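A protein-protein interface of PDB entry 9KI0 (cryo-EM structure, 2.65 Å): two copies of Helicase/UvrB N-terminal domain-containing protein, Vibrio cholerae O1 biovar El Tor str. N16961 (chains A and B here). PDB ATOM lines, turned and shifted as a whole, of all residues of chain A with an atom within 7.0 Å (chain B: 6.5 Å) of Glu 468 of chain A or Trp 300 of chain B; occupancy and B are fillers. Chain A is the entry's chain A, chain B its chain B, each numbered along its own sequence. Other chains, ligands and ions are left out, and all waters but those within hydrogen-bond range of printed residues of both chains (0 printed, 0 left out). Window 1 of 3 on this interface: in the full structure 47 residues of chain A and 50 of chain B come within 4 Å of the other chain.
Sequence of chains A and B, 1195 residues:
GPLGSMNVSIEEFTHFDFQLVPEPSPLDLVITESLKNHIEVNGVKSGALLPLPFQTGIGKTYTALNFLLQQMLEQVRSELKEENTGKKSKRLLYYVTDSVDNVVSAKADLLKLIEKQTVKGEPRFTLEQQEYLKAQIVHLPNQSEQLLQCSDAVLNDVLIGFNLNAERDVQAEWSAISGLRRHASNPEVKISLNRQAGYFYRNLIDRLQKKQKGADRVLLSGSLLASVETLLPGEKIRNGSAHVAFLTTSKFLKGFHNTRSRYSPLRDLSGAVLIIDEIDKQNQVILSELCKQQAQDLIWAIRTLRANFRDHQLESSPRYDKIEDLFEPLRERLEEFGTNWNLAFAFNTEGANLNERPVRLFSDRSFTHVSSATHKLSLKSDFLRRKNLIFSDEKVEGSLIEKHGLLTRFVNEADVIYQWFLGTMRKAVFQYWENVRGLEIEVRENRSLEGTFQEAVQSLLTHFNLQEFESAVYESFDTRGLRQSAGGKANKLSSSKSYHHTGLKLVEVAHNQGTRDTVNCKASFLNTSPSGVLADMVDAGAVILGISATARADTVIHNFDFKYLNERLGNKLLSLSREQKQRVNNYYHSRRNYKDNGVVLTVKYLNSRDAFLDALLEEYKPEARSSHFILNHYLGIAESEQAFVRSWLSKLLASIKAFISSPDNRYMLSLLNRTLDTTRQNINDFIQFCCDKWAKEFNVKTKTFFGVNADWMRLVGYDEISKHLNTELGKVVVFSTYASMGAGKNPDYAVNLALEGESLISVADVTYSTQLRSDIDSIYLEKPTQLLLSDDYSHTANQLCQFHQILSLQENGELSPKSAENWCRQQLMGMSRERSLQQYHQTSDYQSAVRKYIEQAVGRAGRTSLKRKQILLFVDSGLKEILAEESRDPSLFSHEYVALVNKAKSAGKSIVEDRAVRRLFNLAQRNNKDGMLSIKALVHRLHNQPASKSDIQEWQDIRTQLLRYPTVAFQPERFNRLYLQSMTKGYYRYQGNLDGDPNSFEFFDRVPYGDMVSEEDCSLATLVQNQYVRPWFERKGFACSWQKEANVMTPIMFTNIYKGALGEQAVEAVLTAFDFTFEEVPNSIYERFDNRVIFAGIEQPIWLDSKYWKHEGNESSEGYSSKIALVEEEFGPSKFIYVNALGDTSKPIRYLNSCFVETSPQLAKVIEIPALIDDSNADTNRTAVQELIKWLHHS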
ATOM      1  N   GLN A 296     -36.151 -28.173 -33.983  1.00  0.00           N
ATOM      2  CA  GLN A 296     -34.767 -27.742 -33.878  1.00  0.00           C
ATOM      3  C   GLN A 296     -34.498 -26.611 -34.860  1.00  0.00           C
ATOM      4  O   GLN A 296     -34.913 -26.673 -36.019  1.00  0.00           O
ATOM      5  CB  GLN A 296     -33.813 -28.907 -34.149  1.00  0.00           C
ATOM      6  CG  GLN A 296     -32.343 -28.551 -34.046  1.00  0.00           C
ATOM      7  CD  GLN A 296     -31.880 -28.409 -32.614  1.00  0.00           C
ATOM      8  OE1 GLN A 296     -31.528 -29.392 -31.965  1.00  0.00           O
ATOM      9  NE2 GLN A 296     -31.874 -27.182 -32.112  1.00  0.00           N
ATOM     10  N   TRP A 300     -28.917 -22.463 -36.146  1.00  0.00           N
ATOM     11  CA  TRP A 300     -28.133 -22.492 -34.921  1.00  0.00           C
ATOM     12  C   TRP A 300     -27.410 -23.822 -34.777  1.00  0.00           C
ATOM     13  O   TRP A 300     -26.245 -23.857 -34.371  1.00  0.00           O
ATOM     14  CB  TRP A 300     -29.031 -22.234 -33.712  1.00  0.00           C
ATOM     15  CG  TRP A 300     -28.344 -22.497 -32.412  1.00  0.00           C
ATOM     16  CD1 TRP A 300     -27.580 -21.625 -31.698  1.00  0.00           C
ATOM     17  CD2 TRP A 300     -28.336 -23.728 -31.680  1.00  0.00           C
ATOM     18  NE1 TRP A 300     -27.105 -22.231 -30.563  1.00  0.00           N
ATOM     19  CE2 TRP A 300     -27.554 -23.524 -30.532  1.00  0.00           C
ATOM     20  CE3 TRP A 300     -28.918 -24.981 -31.885  1.00  0.00           C
ATOM     21  CZ2 TRP A 300     -27.340 -24.523 -29.590  1.00  0.00           C
ATOM     22  CZ3 TRP A 300     -28.702 -25.972 -30.953  1.00  0.00           C
ATOM     23  CH2 TRP A 300     -27.921 -25.739 -29.820  1.00  0.00           C
ATOM     24  N   THR A 304     -23.394 -24.144 -34.704  1.00  0.00           N
ATOM     25  CA  THR A 304     -22.751 -24.678 -33.510  1.00  0.00           C
ATOM     26  C   THR A 304     -21.882 -25.877 -33.855  1.00  0.00           C
ATOM     27  O   THR A 304     -20.754 -25.999 -33.356  1.00  0.00           O
ATOM     28  CB  THR A 304     -23.811 -25.059 -32.477  1.00  0.00           C
ATOM     29  OG1 THR A 304     -24.636 -23.925 -32.201  1.00  0.00           O
ATOM     30  CG2 THR A 304     -23.171 -25.528 -31.190  1.00  0.00           C
ATOM     31  N   ASN A 308     -17.794 -25.826 -33.196  1.00  0.00           N
ATOM     32  CA  ASN A 308     -17.179 -26.710 -32.214  1.00  0.00           C
ATOM     33  C   ASN A 308     -16.409 -27.877 -32.816  1.00  0.00           C
ATOM     34  O   ASN A 308     -15.534 -28.430 -32.142  1.00  0.00           O
ATOM     35  CB  ASN A 308     -18.238 -27.242 -31.251  1.00  0.00           C
ATOM     36  CG  ASN A 308     -18.766 -26.170 -30.332  1.00  0.00           C
ATOM     37  OD1 ASN A 308     -18.027 -25.615 -29.526  1.00  0.00           O
ATOM     38  ND2 ASN A 308     -20.047 -25.865 -30.451  1.00  0.00           N
ATOM     39  N   LEU A 461     -20.044 -35.669 -25.716  1.00  0.00           N
ATOM     40  CA  LEU A 461     -20.490 -34.292 -25.853  1.00  0.00           C
ATOM     41  C   LEU A 461     -19.639 -33.350 -25.014  1.00  0.00           C
ATOM     42  O   LEU A 461     -19.412 -32.206 -25.416  1.00  0.00           O
ATOM     43  CB  LEU A 461     -21.962 -34.181 -25.475  1.00  0.00           C
ATOM     44  CG  LEU A 461     -22.919 -34.792 -26.499  1.00  0.00           C
ATOM     45  CD1 LEU A 461     -24.332 -34.398 -26.179  1.00  0.00           C
ATOM     46  CD2 LEU A 461     -22.563 -34.379 -27.916  1.00  0.00           C
ATOM     47  N   PHE A 464     -16.430 -32.758 -27.000  1.00  0.00           N
ATOM     48  CA  PHE A 464     -16.607 -31.915 -28.175  1.00  0.00           C
ATOM     49  C   PHE A 464     -17.226 -30.559 -27.857  1.00  0.00           C
ATOM     50  O   PHE A 464     -17.408 -29.755 -28.774  1.00  0.00           O
ATOM     51  CB  PHE A 464     -17.463 -32.632 -29.220  1.00  0.00           C
ATOM     52  CG  PHE A 464     -16.761 -33.766 -29.897  1.00  0.00           C
ATOM     53  CD1 PHE A 464     -15.490 -33.596 -30.413  1.00  0.00           C
ATOM     54  CD2 PHE A 464     -17.373 -34.999 -30.028  1.00  0.00           C
ATOM     55  CE1 PHE A 464     -14.841 -34.634 -31.039  1.00  0.00           C
ATOM     56  CE2 PHE A 464     -16.727 -36.040 -30.655  1.00  0.00           C
ATOM     57  CZ  PHE A 464     -15.460 -35.856 -31.161  1.00  0.00           C
ATOM     58  N   ASN A 465     -17.547 -30.293 -26.590  1.00  0.00           N
ATOM     59  CA  ASN A 465     -18.179 -29.040 -26.164  1.00  0.00           C
ATOM     60  C   ASN A 465     -19.545 -28.852 -26.820  1.00  0.00           C
ATOM     61  O   ASN A 465     -19.955 -27.734 -27.137  1.00  0.00           O
ATOM     62  CB  ASN A 465     -17.273 -27.836 -26.437  1.00  0.00           C
ATOM     63  CG  ASN A 465     -17.537 -26.676 -25.497  1.00  0.00           C
ATOM     64  OD1 ASN A 465     -17.287 -26.763 -24.298  1.00  0.00           O
ATOM     65  ND2 ASN A 465     -18.040 -25.580 -26.043  1.00  0.00           N
ATOM     66  N   LEU A 466     -20.261 -29.951 -27.017  1.00  0.00           N
ATOM     67  CA  LEU A 466     -21.581 -29.940 -27.632  1.00  0.00           C
ATOM     68  C   LEU A 466     -22.639 -30.436 -26.657  1.00  0.00           C
ATOM     69  O   LEU A 466     -23.518 -31.218 -27.015  1.00  0.00           O
ATOM     70  CB  LEU A 466     -21.592 -30.773 -28.909  1.00  0.00           C
ATOM     71  CG  LEU A 466     -20.711 -30.260 -30.045  1.00  0.00           C
ATOM     72  CD1 LEU A 466     -20.475 -31.357 -31.058  1.00  0.00           C
ATOM     73  CD2 LEU A 466     -21.347 -29.053 -30.701  1.00  0.00           C
ATOM     74  N   GLN A 467     -22.562 -29.989 -25.404  1.00  0.00           N
ATOM     75  CA  GLN A 467     -23.533 -30.408 -24.402  1.00  0.00           C
ATOM     76  C   GLN A 467     -24.924 -29.842 -24.647  1.00  0.00           C
ATOM     77  O   GLN A 467     -25.901 -30.411 -24.142  1.00  0.00           O
ATOM     78  CB  GLN A 467     -23.050 -29.982 -23.016  1.00  0.00           C
ATOM     79  CG  GLN A 467     -21.788 -30.681 -22.553  1.00  0.00           C
ATOM     80  CD  GLN A 467     -20.612 -29.734 -22.427  1.00  0.00           C
ATOM     81  OE1 GLN A 467     -20.247 -29.050 -23.379  1.00  0.00           O
ATOM     82  NE2 GLN A 467     -20.014 -29.687 -21.246  1.00  0.00           N
ATOM     83  N   GLU A 468     -25.057 -28.856 -25.531  1.00  0.00           N
ATOM     84  CA  GLU A 468     -26.366 -28.300 -25.833  1.00  0.00           C
ATOM     85  C   GLU A 468     -27.174 -29.210 -26.734  1.00  0.00           C
ATOM     86  O   GLU A 468     -28.376 -28.985 -26.904  1.00  0.00           O
ATOM     87  CB  GLU A 468     -26.219 -26.922 -26.487  1.00  0.00           C
ATOM     88  CG  GLU A 468     -24.997 -26.773 -27.387  1.00  0.00           C
ATOM     89  CD  GLU A 468     -23.747 -26.352 -26.631  1.00  0.00           C
ATOM     90  OE1 GLU A 468     -23.644 -26.662 -25.427  1.00  0.00           O
ATOM     91  OE2 GLU A 468     -22.864 -25.712 -27.243  1.00  0.00           O
ATOM     92  N   PHE A 469     -26.542 -30.223 -27.311  1.00  0.00           N
ATOM     93  CA  PHE A 469     -27.238 -31.231 -28.083  1.00  0.00           C
ATOM     94  C   PHE A 469     -27.581 -32.445 -27.239  1.00  0.00           C
ATOM     95  O   PHE A 469     -28.126 -33.417 -27.775  1.00  0.00           O
ATOM     96  CB  PHE A 469     -26.381 -31.672 -29.270  1.00  0.00           C
ATOM     97  CG  PHE A 469     -26.305 -30.668 -30.378  1.00  0.00           C
ATOM     98  CD1 PHE A 469     -27.385 -30.451 -31.210  1.00  0.00           C
ATOM     99  CD2 PHE A 469     -25.146 -29.946 -30.593  1.00  0.00           C
ATOM    100  CE1 PHE A 469     -27.313 -29.532 -32.231  1.00  0.00           C
ATOM    101  CE2 PHE A 469     -25.069 -29.025 -31.612  1.00  0.00           C
ATOM    102  CZ  PHE A 469     -26.154 -28.818 -32.432  1.00  0.00           C
ATOM    103  N   GLU A 470     -27.363 -32.381 -25.918  1.00  0.00           N
ATOM    104  CA  GLU A 470     -27.549 -33.581 -25.107  1.00  0.00           C
ATOM    105  C   GLU A 470     -28.985 -34.077 -25.166  1.00  0.00           C
ATOM    106  O   GLU A 470     -29.226 -35.251 -25.478  1.00  0.00           O
ATOM    107  CB  GLU A 470     -27.135 -33.302 -23.664  1.00  0.00           C
ATOM    108  CG  GLU A 470     -27.589 -34.350 -22.669  1.00  0.00           C
ATOM    109  CD  GLU A 470     -27.920 -33.760 -21.314  1.00  0.00           C
ATOM    110  OE1 GLU A 470     -27.294 -34.176 -20.316  1.00  0.00           O
ATOM    111  OE2 GLU A 470     -28.804 -32.880 -21.243  1.00  0.00           O
ATOM    112  N   SER A 471     -29.951 -33.165 -25.052  1.00  0.00           N
ATOM    113  CA  SER A 471     -31.342 -33.582 -25.146  1.00  0.00           C
ATOM    114  C   SER A 471     -31.624 -34.140 -26.529  1.00  0.00           C
ATOM    115  O   SER A 471     -32.227 -35.210 -26.664  1.00  0.00           O
ATOM    116  CB  SER A 471     -32.269 -32.409 -24.834  1.00  0.00           C
ATOM    117  OG  SER A 471     -31.764 -31.201 -25.376  1.00  0.00           O
ATOM    118  N   ALA A 472     -31.094 -33.483 -27.561  1.00  0.00           N
ATOM    119  CA  ALA A 472     -31.334 -33.948 -28.917  1.00  0.00           C
ATOM    120  C   ALA A 472     -30.768 -35.344 -29.099  1.00  0.00           C
ATOM    121  O   ALA A 472     -31.354 -36.175 -29.801  1.00  0.00           O
ATOM    122  CB  ALA A 472     -30.721 -32.978 -29.926  1.00  0.00           C
ATOM    123  N   VAL A 473     -29.617 -35.619 -28.484  1.00  0.00           N
ATOM    124  CA  VAL A 473     -29.033 -36.945 -28.624  1.00  0.00           C
ATOM    125  C   VAL A 473     -29.880 -37.977 -27.888  1.00  0.00           C
ATOM    126  O   VAL A 473     -30.035 -39.112 -28.350  1.00  0.00           O
ATOM    127  CB  VAL A 473     -27.572 -36.947 -28.142  1.00  0.00           C
ATOM    128  CG1 VAL A 473     -27.001 -38.351 -28.190  1.00  0.00           C
ATOM    129  CG2 VAL A 473     -26.740 -36.017 -29.004  1.00  0.00           C
ATOM    130  N   GLN B 296     -21.916 -21.013 -13.110  1.00  0.00           N
ATOM    131  CA  GLN B 296     -21.542 -21.155 -14.508  1.00  0.00           C
ATOM    132  C   GLN B 296     -20.308 -22.035 -14.632  1.00  0.00           C
ATOM    133  O   GLN B 296     -19.345 -21.868 -13.880  1.00  0.00           O
ATOM    134  CB  GLN B 296     -21.274 -19.785 -15.136  1.00  0.00           C
ATOM    135  CG  GLN B 296     -20.928 -19.831 -16.613  1.00  0.00           C
ATOM    136  CD  GLN B 296     -22.136 -20.091 -17.486  1.00  0.00           C
ATOM    137  OE1 GLN B 296     -22.823 -19.162 -17.904  1.00  0.00           O
ATOM    138  NE2 GLN B 296     -22.397 -21.359 -17.769  1.00  0.00           N
ATOM    139  N   ASP B 297     -20.342 -22.971 -15.578  1.00  0.00           N
ATOM    140  CA  ASP B 297     -19.172 -23.776 -15.911  1.00  0.00           C
ATOM    141  C   ASP B 297     -18.215 -22.911 -16.720  1.00  0.00           C
ATOM    142  O   ASP B 297     -18.529 -22.513 -17.844  1.00  0.00           O
ATOM    143  CB  ASP B 297     -19.583 -25.022 -16.689  1.00  0.00           C
ATOM    144  CG  ASP B 297     -18.427 -25.974 -16.924  1.00  0.00           C
ATOM    145  OD1 ASP B 297     -17.360 -25.785 -16.307  1.00  0.00           O
ATOM    146  OD2 ASP B 297     -18.584 -26.915 -17.728  1.00  0.00           O
ATOM    147  N   LEU B 298     -17.047 -22.613 -16.151  1.00  0.00           N
ATOM    148  CA  LEU B 298     -16.140 -21.672 -16.795  1.00  0.00           C
ATOM    149  C   LEU B 298     -15.418 -22.287 -17.983  1.00  0.00           C
ATOM    150  O   LEU B 298     -15.118 -21.579 -18.954  1.00  0.00           O
ATOM    151  CB  LEU B 298     -15.126 -21.151 -15.777  1.00  0.00           C
ATOM    152  CG  LEU B 298     -15.526 -19.893 -15.008  1.00  0.00           C
ATOM    153  CD1 LEU B 298     -14.392 -19.439 -14.113  1.00  0.00           C
ATOM    154  CD2 LEU B 298     -15.933 -18.790 -15.967  1.00  0.00           C
ATOM    155  N   ILE B 299     -15.184 -23.599 -17.960  1.00  0.00           N
ATOM    156  CA  ILE B 299     -14.520 -24.241 -19.088  1.00  0.00           C
ATOM    157  C   ILE B 299     -15.442 -24.266 -20.296  1.00  0.00           C
ATOM    158  O   ILE B 299     -15.040 -23.899 -21.408  1.00  0.00           O
ATOM    159  CB  ILE B 299     -14.063 -25.658 -18.701  1.00  0.00           C
ATOM    160  CG1 ILE B 299     -12.974 -25.598 -17.632  1.00  0.00           C
ATOM    161  CG2 ILE B 299     -13.556 -26.402 -19.922  1.00  0.00           C
ATOM    162  CD1 ILE B 299     -12.601 -26.949 -17.075  1.00  0.00           C
ATOM    163  N   TRP B 300     -16.707 -24.634 -20.090  1.00  0.00           N
ATOM    164  CA  TRP B 300     -17.654 -24.630 -21.195  1.00  0.00           C
ATOM    165  C   TRP B 300     -17.875 -23.216 -21.705  1.00  0.00           C
ATOM    166  O   TRP B 300     -17.952 -22.991 -22.917  1.00  0.00           O
ATOM    167  CB  TRP B 300     -18.978 -25.259 -20.764  1.00  0.00           C
ATOM    168  CG  TRP B 300     -20.060 -25.072 -21.777  1.00  0.00           C
ATOM    169  CD1 TRP B 300     -20.325 -25.871 -22.846  1.00  0.00           C
ATOM    170  CD2 TRP B 300     -21.008 -24.003 -21.830  1.00  0.00           C
ATOM    171  NE1 TRP B 300     -21.385 -25.372 -23.558  1.00  0.00           N
ATOM    172  CE2 TRP B 300     -21.821 -24.222 -22.955  1.00  0.00           C
ATOM    173  CE3 TRP B 300     -21.251 -22.881 -21.033  1.00  0.00           C
ATOM    174  CZ2 TRP B 300     -22.859 -23.365 -23.301  1.00  0.00           C
ATOM    175  CZ3 TRP B 300     -22.277 -22.031 -21.380  1.00  0.00           C
ATOM    176  CH2 TRP B 300     -23.070 -22.277 -22.503  1.00  0.00           C
ATOM    177  N   ALA B 301     -17.954 -22.245 -20.795  1.00  0.00           N
ATOM    178  CA  ALA B 301     -18.255 -20.878 -21.203  1.00  0.00           C
ATOM    179  C   ALA B 301     -17.113 -20.290 -22.019  1.00  0.00           C
ATOM    180  O   ALA B 301     -17.348 -19.623 -23.032  1.00  0.00           O
ATOM    181  CB  ALA B 301     -18.543 -20.012 -19.978  1.00  0.00           C
ATOM    182  N   ILE B 302     -15.869 -20.587 -21.642  1.00  0.00           N
ATOM    183  CA  ILE B 302     -14.759 -19.999 -22.379  1.00  0.00           C
ATOM    184  C   ILE B 302     -14.524 -20.748 -23.685  1.00  0.00           C
ATOM    185  O   ILE B 302     -14.184 -20.129 -24.701  1.00  0.00           O
ATOM    186  CB  ILE B 302     -13.494 -19.961 -21.504  1.00  0.00           C
ATOM    187  CG1 ILE B 302     -13.728 -19.081 -20.277  1.00  0.00           C
ATOM    188  CG2 ILE B 302     -12.313 -19.418 -22.282  1.00  0.00           C
ATOM    189  CD1 ILE B 302     -14.161 -17.680 -20.613  1.00  0.00           C
ATOM    190  N   ARG B 303     -14.776 -22.061 -23.720  1.00  0.00           N
ATOM    191  CA  ARG B 303     -14.651 -22.783 -24.980  1.00  0.00           C
ATOM    192  C   ARG B 303     -15.746 -22.377 -25.959  1.00  0.00           C
ATOM    193  O   ARG B 303     -15.499 -22.296 -27.170  1.00  0.00           O
ATOM    194  CB  ARG B 303     -14.690 -24.288 -24.721  1.00  0.00           C
ATOM    195  CG  ARG B 303     -13.515 -24.807 -23.912  1.00  0.00           C
ATOM    196  CD  ARG B 303     -12.872 -26.025 -24.536  1.00  0.00           C
ATOM    197  NE  ARG B 303     -13.697 -27.216 -24.391  1.00  0.00           N
ATOM    198  CZ  ARG B 303     -13.449 -28.375 -24.982  1.00  0.00           C
ATOM    199  NH1 ARG B 303     -12.375 -28.555 -25.730  1.00  0.00           N
ATOM    200  NH2 ARG B 303     -14.297 -29.384 -24.813  1.00  0.00           N
ATOM    201  N   THR B 304     -16.937 -22.050 -25.451  1.00  0.00           N
ATOM    202  CA  THR B 304     -18.015 -21.591 -26.317  1.00  0.00           C
ATOM    203  C   THR B 304     -17.738 -20.186 -26.825  1.00  0.00           C
ATOM    204  O   THR B 304     -17.946 -19.899 -28.010  1.00  0.00           O
ATOM    205  CB  THR B 304     -19.346 -21.640 -25.568  1.00  0.00           C
ATOM    206  OG1 THR B 304     -19.640 -22.994 -25.208  1.00  0.00           O
ATOM    207  CG2 THR B 304     -20.471 -21.106 -26.431  1.00  0.00           C
ATOM    208  N   LEU B 305     -17.270 -19.293 -25.950  1.00  0.00           N
ATOM    209  CA  LEU B 305     -16.961 -17.939 -26.390  1.00  0.00           C
ATOM    210  C   LEU B 305     -15.850 -17.950 -27.429  1.00  0.00           C
ATOM    211  O   LEU B 305     -15.886 -17.182 -28.393  1.00  0.00           O
ATOM    212  CB  LEU B 305     -16.566 -17.073 -25.196  1.00  0.00           C
ATOM    213  CG  LEU B 305     -17.692 -16.595 -24.281  1.00  0.00           C
ATOM    214  CD1 LEU B 305     -17.120 -15.911 -23.053  1.00  0.00           C
ATOM    215  CD2 LEU B 305     -18.621 -15.668 -25.034  1.00  0.00           C
ATOM    216  N   ASN B 308     -17.263 -19.493 -30.927  1.00  0.00           N
ATOM    217  CA  ASN B 308     -18.236 -18.678 -31.643  1.00  0.00           C
ATOM    218  C   ASN B 308     -17.761 -17.259 -31.925  1.00  0.00           C
ATOM    219  O   ASN B 308     -18.530 -16.465 -32.473  1.00  0.00           O
ATOM    220  CB  ASN B 308     -19.552 -18.634 -30.867  1.00  0.00           C
ATOM    221  CG  ASN B 308     -20.288 -19.949 -30.905  1.00  0.00           C
ATOM    222  OD1 ASN B 308     -20.648 -20.440 -31.971  1.00  0.00           O
ATOM    223  ND2 ASN B 308     -20.511 -20.534 -29.739  1.00  0.00           N
ATOM    224  N   GLU B 468     -27.029 -19.373 -25.957  1.00  0.00           N
ATOM    225  CA  GLU B 468     -26.969 -20.117 -24.706  1.00  0.00           C
ATOM    226  C   GLU B 468     -26.609 -19.223 -23.534  1.00  0.00           C
ATOM    227  O   GLU B 468     -26.785 -19.628 -22.382  1.00  0.00           O
ATOM    228  CB  GLU B 468     -25.959 -21.257 -24.816  1.00  0.00           C
ATOM    229  CG  GLU B 468     -25.877 -21.891 -26.196  1.00  0.00           C
ATOM    230  CD  GLU B 468     -24.841 -21.225 -27.081  1.00  0.00           C
ATOM    231  OE1 GLU B 468     -23.809 -20.770 -26.549  1.00  0.00           O
ATOM    232  OE2 GLU B 468     -25.060 -21.157 -28.310  1.00  0.00           O
ATOM    233  N   PHE B 469     -26.106 -18.026 -23.803  1.00  0.00           N
ATOM    234  CA  PHE B 469     -25.811 -17.056 -22.767  1.00  0.00           C
ATOM    235  C   PHE B 469     -26.983 -16.119 -22.525  1.00  0.00           C
ATOM    236  O   PHE B 469     -26.867 -15.208 -21.699  1.00  0.00           O
ATOM    237  CB  PHE B 469     -24.574 -16.241 -23.146  1.00  0.00           C
ATOM    238  CG  PHE B 469     -23.287 -16.998 -23.018  1.00  0.00           C
ATOM    239  CD1 PHE B 469     -22.760 -17.291 -21.775  1.00  0.00           C
ATOM    240  CD2 PHE B 469     -22.604 -17.416 -24.146  1.00  0.00           C
ATOM    241  CE1 PHE B 469     -21.577 -17.987 -21.660  1.00  0.00           C
ATOM    242  CE2 PHE B 469     -21.422 -18.111 -24.035  1.00  0.00           C
ATOM    243  CZ  PHE B 469     -20.908 -18.396 -22.792  1.00  0.00           C
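Printed residues of chain B within 4 Å of Trp 300 of chain A: Glu 468 (3.2 Å). Printed residues of chain B within 4 Å of Gln 467 of chain A: Trp 300. Of chain B, only Trp 300 (3.2 Å) comes within 4 Å of Glu 468 of chain A. Ala 472 of chain A touches none of the printed residues of chain B. Trp 300 of chain B touches three residues of chain A. Ile 302 of chain B touches none of the printed residues of chain A. Printed residues of chain A within 4 Å of Arg 303 of chain B: Asn 465 (3.6 Å). Printed residues of chain A within 4 Å of Thr 304 of chain B: Asn 465 (3.2 Å). The nearest residue of chain B that does not touch Glu 468 of chain A is Thr 304 of chain B (4.7 Å). The nearest printed residue of chain B that does not touch Asn 465 of chain A is Ile 299 of chain B (4.6 Å).
Trp 300 of chain A touches Glu 468 of chain B, and with the chains exchanged Glu 468 of chain A touches Trp 300 of chain B. 6 positions are printed for both chains. Of the 6 pairs that touch across the chains among the printed residues, 2 have their exchanged pair printed and touching as well.
Asn 465 of chain A touches Trp 300 of chain B. Asn 465 of chain A touches Arg 303 of chain B. CD1 of Trp 300 of chain B touches OE1 of Gln 467 of chain A, 3.2 Å away.
O of Thr 304 of chain B is in hydrogen-bond range of ND2 of Asn 308 of chain B (3.2 Å). The side-chain hydroxyl of Thr 304 of chain A is in hydrogen-bond range of the backbone carbonyl oxygen of Trp 300 of chain A, 2.7 Å away. The side-chain hydroxyl (OG1) of Thr 304 of chain B is in hydrogen-bond range of the backbone carbonyl oxygen (O) of Trp 300 of chain B. The side-chain amide oxygen (OD1) of Asn 308 of chain A sits at hydrogen-bond distance from the side-chain amide nitrogen (ND2) of Asn 465 of chain A, 3.5 Å away.
ND2 of Asn 465 of chain A is in hydrogen-bond range of OG1 of Thr 304 of chain B, 3.2 Å away. The indole nitrogen (NE1) of Trp 300 of chain A sits at hydrogen-bond distance from the side-chain carboxylate (OE2) of Glu 468 of chain B (3.2 Å). The side-chain carboxylate (OE1) of Glu 468 of chain A sits at hydrogen-bond distance from the indole nitrogen (NE1) of Trp 300 of chain B, 3.2 Å away.
Of the 15 printed residues of chain A, 4 touch a printed residue of chain B. Hydrophobic or aromatic side chains of chain A within 4 Å of the printed part of chain B: Trp 300. Hydrophobic or aromatic side chains of chain B within 4 Å of the printed part of chain A: Trp 300. Among the printed residues, no Asp or Glu carboxylate lies within 4 Å of a Lys or Arg side-chain nitrogen of the other chain.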
